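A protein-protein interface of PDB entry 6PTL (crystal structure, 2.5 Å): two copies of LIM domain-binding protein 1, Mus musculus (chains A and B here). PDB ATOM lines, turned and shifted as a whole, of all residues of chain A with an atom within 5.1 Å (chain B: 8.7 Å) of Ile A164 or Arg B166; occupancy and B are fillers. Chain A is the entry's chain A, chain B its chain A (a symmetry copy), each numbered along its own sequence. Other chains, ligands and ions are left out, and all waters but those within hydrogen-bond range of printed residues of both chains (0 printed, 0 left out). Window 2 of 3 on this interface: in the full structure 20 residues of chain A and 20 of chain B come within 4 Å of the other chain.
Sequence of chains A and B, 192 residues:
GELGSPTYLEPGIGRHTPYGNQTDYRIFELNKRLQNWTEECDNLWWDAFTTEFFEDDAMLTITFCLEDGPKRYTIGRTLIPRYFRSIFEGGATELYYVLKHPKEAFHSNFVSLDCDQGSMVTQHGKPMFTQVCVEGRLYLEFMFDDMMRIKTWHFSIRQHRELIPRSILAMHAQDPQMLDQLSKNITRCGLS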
ATOM      1  N   THR A 130     -12.484   2.213   6.120  1.00  0.00           N
ATOM      2  CA  THR A 130     -13.582   2.181   7.126  1.00  0.00           C
ATOM      3  C   THR A 130     -14.916   2.488   6.436  1.00  0.00           C
ATOM      4  O   THR A 130     -14.895   3.065   5.330  1.00  0.00           O
ATOM      5  CB  THR A 130     -13.297   3.119   8.308  1.00  0.00           C
ATOM      6  OG1 THR A 130     -14.389   3.021   9.223  1.00  0.00           O
ATOM      7  CG2 THR A 130     -13.106   4.567   7.909  1.00  0.00           C
ATOM      8  N   GLU A 162     -19.452   4.084  12.986  1.00  0.00           N
ATOM      9  CA  GLU A 162     -18.229   3.878  12.163  1.00  0.00           C
ATOM     10  C   GLU A 162     -17.743   2.438  12.364  1.00  0.00           C
ATOM     11  O   GLU A 162     -17.393   2.091  13.509  1.00  0.00           O
ATOM     12  CB  GLU A 162     -17.133   4.873  12.555  1.00  0.00           C
ATOM     13  CG  GLU A 162     -17.561   6.328  12.457  1.00  0.00           C
ATOM     14  CD  GLU A 162     -16.460   7.345  12.706  1.00  0.00           C
ATOM     15  OE1 GLU A 162     -16.791   8.528  12.924  1.00  0.00           O
ATOM     16  OE2 GLU A 162     -15.274   6.959  12.678  1.00  0.00           O
ATOM     17  N   LEU A 163     -17.740   1.633  11.296  1.00  0.00           N
ATOM     18  CA  LEU A 163     -17.282   0.217  11.307  1.00  0.00           C
ATOM     19  C   LEU A 163     -15.873   0.141  10.713  1.00  0.00           C
ATOM     20  O   LEU A 163     -15.667   0.684   9.609  1.00  0.00           O
ATOM     21  CB  LEU A 163     -18.264  -0.646  10.507  1.00  0.00           C
ATOM     22  CG  LEU A 163     -19.739  -0.506  10.882  1.00  0.00           C
ATOM     23  CD1 LEU A 163     -20.592  -1.474  10.078  1.00  0.00           C
ATOM     24  CD2 LEU A 163     -19.954  -0.722  12.373  1.00  0.00           C
ATOM     25  N   ILE A 164     -14.950  -0.513  11.427  1.00  0.00           N
ATOM     26  CA  ILE A 164     -13.521  -0.689  11.029  1.00  0.00           C
ATOM     27  C   ILE A 164     -13.283  -2.177  10.784  1.00  0.00           C
ATOM     28  O   ILE A 164     -13.843  -3.017  11.487  1.00  0.00           O
ATOM     29  CB  ILE A 164     -12.582  -0.101  12.106  1.00  0.00           C
ATOM     30  CG1 ILE A 164     -12.891   1.376  12.367  1.00  0.00           C
ATOM     31  CG2 ILE A 164     -11.117  -0.300  11.744  1.00  0.00           C
ATOM     32  CD1 ILE A 164     -12.311   1.910  13.656  1.00  0.00           C
ATOM     33  N   PRO A 165     -12.461  -2.549   9.774  1.00  0.00           N
ATOM     34  CA  PRO A 165     -12.228  -3.955   9.439  1.00  0.00           C
ATOM     35  C   PRO A 165     -11.551  -4.759  10.558  1.00  0.00           C
ATOM     36  O   PRO A 165     -11.074  -4.165  11.510  1.00  0.00           O
ATOM     37  CB  PRO A 165     -11.275  -3.918   8.236  1.00  0.00           C
ATOM     38  CG  PRO A 165     -11.374  -2.509   7.712  1.00  0.00           C
ATOM     39  CD  PRO A 165     -11.721  -1.637   8.893  1.00  0.00           C
ATOM     40  N   ARG A 166     -11.515  -6.084  10.396  1.00  0.00           N
ATOM     41  CA  ARG A 166     -10.821  -7.023  11.314  1.00  0.00           C
ATOM     42  C   ARG A 166      -9.325  -7.050  10.968  1.00  0.00           C
ATOM     43  O   ARG A 166      -8.526  -7.414  11.854  1.00  0.00           O
ATOM     44  CB  ARG A 166     -11.452  -8.417  11.235  1.00  0.00           C
ATOM     45  CG  ARG A 166     -11.375  -9.197  12.539  1.00  0.00           C
ATOM     46  CD  ARG A 166     -11.861 -10.627  12.402  1.00  0.00           C
ATOM     47  NE  ARG A 166     -11.662 -11.381  13.633  1.00  0.00           N
ATOM     48  CZ  ARG A 166     -11.864 -12.689  13.771  1.00  0.00           C
ATOM     49  NH1 ARG A 166     -11.648 -13.268  14.941  1.00  0.00           N
ATOM     50  NH2 ARG A 166     -12.276 -13.419  12.747  1.00  0.00           N
ATOM     51  N   PHE B 129     -22.531  -7.428  17.021  1.00  0.00           N
ATOM     52  CA  PHE B 129     -22.899  -6.178  16.303  1.00  0.00           C
ATOM     53  C   PHE B 129     -21.884  -5.926  15.177  1.00  0.00           C
ATOM     54  O   PHE B 129     -21.426  -4.781  15.015  1.00  0.00           O
ATOM     55  CB  PHE B 129     -22.996  -5.022  17.306  1.00  0.00           C
ATOM     56  CG  PHE B 129     -23.327  -3.673  16.717  1.00  0.00           C
ATOM     57  CD1 PHE B 129     -24.588  -3.393  16.219  1.00  0.00           C
ATOM     58  CD2 PHE B 129     -22.371  -2.673  16.677  1.00  0.00           C
ATOM     59  CE1 PHE B 129     -24.874  -2.150  15.675  1.00  0.00           C
ATOM     60  CE2 PHE B 129     -22.652  -1.431  16.130  1.00  0.00           C
ATOM     61  CZ  PHE B 129     -23.905  -1.170  15.634  1.00  0.00           C
ATOM     62  N   THR B 130     -21.543  -6.974  14.417  1.00  0.00           N
ATOM     63  CA  THR B 130     -20.542  -6.933  13.315  1.00  0.00           C
ATOM     64  C   THR B 130     -21.261  -7.058  11.966  1.00  0.00           C
ATOM     65  O   THR B 130     -22.413  -7.533  11.948  1.00  0.00           O
ATOM     66  CB  THR B 130     -19.447  -7.995  13.503  1.00  0.00           C
ATOM     67  OG1 THR B 130     -18.531  -7.881  12.414  1.00  0.00           O
ATOM     68  CG2 THR B 130     -19.974  -9.412  13.569  1.00  0.00           C
ATOM     69  N   GLN B 131     -20.595  -6.626  10.891  1.00  0.00           N
ATOM     70  CA  GLN B 131     -21.103  -6.661   9.492  1.00  0.00           C
ATOM     71  C   GLN B 131     -20.093  -7.415   8.620  1.00  0.00           C
ATOM     72  O   GLN B 131     -18.896  -7.071   8.677  1.00  0.00           O
ATOM     73  CB  GLN B 131     -21.336  -5.237   8.982  1.00  0.00           C
ATOM     74  CG  GLN B 131     -21.540  -5.145   7.474  1.00  0.00           C
ATOM     75  CD  GLN B 131     -22.068  -3.800   7.038  1.00  0.00           C
ATOM     76  OE1 GLN B 131     -22.915  -3.198   7.694  1.00  0.00           O
ATOM     77  NE2 GLN B 131     -21.571  -3.319   5.910  1.00  0.00           N
ATOM     78  N   ARG B 161     -14.667  -9.916   3.907  1.00  0.00           N
ATOM     79  CA  ARG B 161     -14.377  -8.794   4.842  1.00  0.00           C
ATOM     80  C   ARG B 161     -15.388  -8.799   5.994  1.00  0.00           C
ATOM     81  O   ARG B 161     -16.602  -8.791   5.712  1.00  0.00           O
ATOM     82  CB  ARG B 161     -14.420  -7.460   4.089  1.00  0.00           C
ATOM     83  CG  ARG B 161     -13.299  -7.289   3.074  1.00  0.00           C
ATOM     84  CD  ARG B 161     -13.626  -6.268   2.002  1.00  0.00           C
ATOM     85  NE  ARG B 161     -12.456  -5.938   1.196  1.00  0.00           N
ATOM     86  CZ  ARG B 161     -12.399  -4.967   0.285  1.00  0.00           C
ATOM     87  NH1 ARG B 161     -13.452  -4.203   0.048  1.00  0.00           N
ATOM     88  NH2 ARG B 161     -11.277  -4.758  -0.382  1.00  0.00           N
ATOM     89  N   GLU B 162     -14.893  -8.816   7.236  1.00  0.00           N
ATOM     90  CA  GLU B 162     -15.690  -8.648   8.482  1.00  0.00           C
ATOM     91  C   GLU B 162     -15.359  -7.281   9.091  1.00  0.00           C
ATOM     92  O   GLU B 162     -14.187  -7.071   9.458  1.00  0.00           O
ATOM     93  CB  GLU B 162     -15.386  -9.769   9.480  1.00  0.00           C
ATOM     94  CG  GLU B 162     -15.615 -11.164   8.925  1.00  0.00           C
ATOM     95  CD  GLU B 162     -15.455 -12.295   9.930  1.00  0.00           C
ATOM     96  OE1 GLU B 162     -15.344 -13.458   9.492  1.00  0.00           O
ATOM     97  OE2 GLU B 162     -15.444 -12.015  11.145  1.00  0.00           O
ATOM     98  N   LEU B 163     -16.351  -6.389   9.178  1.00  0.00           N
ATOM     99  CA  LEU B 163     -16.212  -5.025   9.759  1.00  0.00           C
ATOM    100  C   LEU B 163     -16.793  -5.023  11.176  1.00  0.00           C
ATOM    101  O   LEU B 163     -17.941  -5.482  11.345  1.00  0.00           O
ATOM    102  CB  LEU B 163     -16.935  -4.010   8.867  1.00  0.00           C
ATOM    103  CG  LEU B 163     -16.578  -4.050   7.381  1.00  0.00           C
ATOM    104  CD1 LEU B 163     -17.295  -2.942   6.626  1.00  0.00           C
ATOM    105  CD2 LEU B 163     -15.074  -3.949   7.169  1.00  0.00           C
ATOM    106  N   ILE B 164     -16.021  -4.521  12.146  1.00  0.00           N
ATOM    107  CA  ILE B 164     -16.397  -4.439  13.588  1.00  0.00           C
ATOM    108  C   ILE B 164     -16.508  -2.962  13.960  1.00  0.00           C
ATOM    109  O   ILE B 164     -15.734  -2.141  13.470  1.00  0.00           O
ATOM    110  CB  ILE B 164     -15.375  -5.201  14.460  1.00  0.00           C
ATOM    111  CG1 ILE B 164     -15.247  -6.662  14.018  1.00  0.00           C
ATOM    112  CG2 ILE B 164     -15.713  -5.102  15.941  1.00  0.00           C
ATOM    113  CD1 ILE B 164     -14.010  -7.358  14.534  1.00  0.00           C
ATOM    114  N   PRO B 165     -17.478  -2.577  14.823  1.00  0.00           N
ATOM    115  CA  PRO B 165     -17.685  -1.172  15.184  1.00  0.00           C
ATOM    116  C   PRO B 165     -16.497  -0.536  15.918  1.00  0.00           C
ATOM    117  O   PRO B 165     -15.600  -1.252  16.330  1.00  0.00           O
ATOM    118  CB  PRO B 165     -18.884  -1.188  16.142  1.00  0.00           C
ATOM    119  CG  PRO B 165     -19.532  -2.531  15.925  1.00  0.00           C
ATOM    120  CD  PRO B 165     -18.435  -3.469  15.489  1.00  0.00           C
ATOM    121  N   ARG B 166     -16.540   0.790  16.073  1.00  0.00           N
ATOM    122  CA  ARG B 166     -15.539   1.578  16.837  1.00  0.00           C
ATOM    123  C   ARG B 166     -15.877   1.502  18.333  1.00  0.00           C
ATOM    124  O   ARG B 166     -14.960   1.713  19.152  1.00  0.00           O
ATOM    125  CB  ARG B 166     -15.495   3.024  16.333  1.00  0.00           C
ATOM    126  CG  ARG B 166     -14.127   3.676  16.466  1.00  0.00           C
ATOM    127  CD  ARG B 166     -14.136   5.149  16.110  1.00  0.00           C
ATOM    128  NE  ARG B 166     -12.842   5.770  16.362  1.00  0.00           N
ATOM    129  CZ  ARG B 166     -12.588   7.074  16.276  1.00  0.00           C
ATOM    130  NH1 ARG B 166     -11.370   7.525  16.529  1.00  0.00           N
ATOM    131  NH2 ARG B 166     -13.544   7.926  15.941  1.00  0.00           N
ATOM    132  N   SER B 167     -17.140   1.207  18.669  1.00  0.00           N
ATOM    133  CA  SER B 167     -17.640   0.998  20.055  1.00  0.00           C
ATOM    134  C   SER B 167     -17.708  -0.503  20.359  1.00  0.00           C
ATOM    135  O   SER B 167     -16.692  -1.145  20.628  1.00  0.00           O
ATOM    136  CB  SER B 167     -18.982   1.658  20.254  1.00  0.00           C
ATOM    137  OG  SER B 167     -19.983   1.026  19.470  1.00  0.00           O
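Leu A163 touches its own counterpart, Leu B163.
Leu A163 touches Ile B164, and with the chains exchanged Ile A164 touches Leu B163.
Ile B164 touches its own counterpart, Ile A164.
Ile A164 touches Arg B166, and with the chains exchanged Arg A166 touches Ile B164.
Positions printed for both chains: 130, 162, 163, 164, 165 and 166.
Of the 13 pairs that touch across the chains among the printed residues, 12 have their exchanged pair printed and touching as well.
OE2 of Glu A162 lies within salt-bridge range of NH2 of Arg B166 (3.8 Å).
The backbone NH of Ile A164 lies within hydrogen-bond range of the backbone carbonyl oxygen of Ile B164 (2.7 Å).
NH2 of Arg A166 is in salt-bridge range of OE2 of Glu B162 (3.8 Å).
Along chain B the printed residues that touch a printed residue of chain A span positions 131 to 166.
Of the 6 printed residues of chain A, 5 touch a printed residue of chain B.
Among the printed residues, 13 pairs touch across the chains.
Among the printed residues, Asp or Glu carboxylates within 4 Å of a Lys or Arg side-chain nitrogen of the other chain: Glu A162 with Arg B166 and Arg A166 with Glu B162.
The backbone carbonyl oxygen (O) of Leu A163 lies within hydrogen-bond range of the side-chain hydroxyl (OG1) of Thr A130 (2.7 Å).
The backbone carbonyl oxygen (O) of Leu B163 lies within hydrogen-bond range of the side-chain hydroxyl (OG1) of Thr B130 (2.7 Å).
N of Leu B163 is in hydrogen-bond range of O of Gln B131 (2.7 Å).
Ile A164 touches just these residues of chain B: Leu B163 (3.6 Å), Ile B164 (2.7 Å) and Arg B166 (3.8 Å).
Printed residues of chain A within 4 Å of Gln B131: Leu A163 (3.7 Å).
Arg B161 touches none of the printed residues of chain A.
Of the printed residues of chain A, Glu B162 touches Pro A165 (3.7 Å) and Arg A166 (3.0 Å).
Of the printed residues of chain A, Leu B163 touches Leu A163, Ile A164 and Pro A165.
Of the printed residues of chain A, Ile B164 touches Leu A163, Ile A164 and Arg A166.
Printed residues of chain A within 4 Å of Pro B165: Glu A162 and Leu A163.
Arg B166 touches just these residues of chain A: Glu A162 (3.0 Å) and Ile A164 (3.8 Å).
The nearest residue of chain B that does not touch Ile A164 is Glu B162 (4.5 Å).
O of Glu A162 touches C of Pro B165 (3.7 Å).
CD1 of Leu A163 touches OE1 of Gln B131, at 3.7 Å.
Leu A163 touches Leu B163 (CB to CB, 3.97 Å).
Leu A163 touches Ile B164 (CA to O, 3.6 Å).
Leu A163 touches Pro B165.
Leu B163 touches Ile A164.
Arg B166 touches Ile A164.
O of Glu B162 touches C of Pro A165 (3.7 Å).
CA of Pro A165 touches CD2 of Leu B163 (3.6 Å).
Arg A166 touches Ile B164 (CG to CD1, 3.8 Å).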
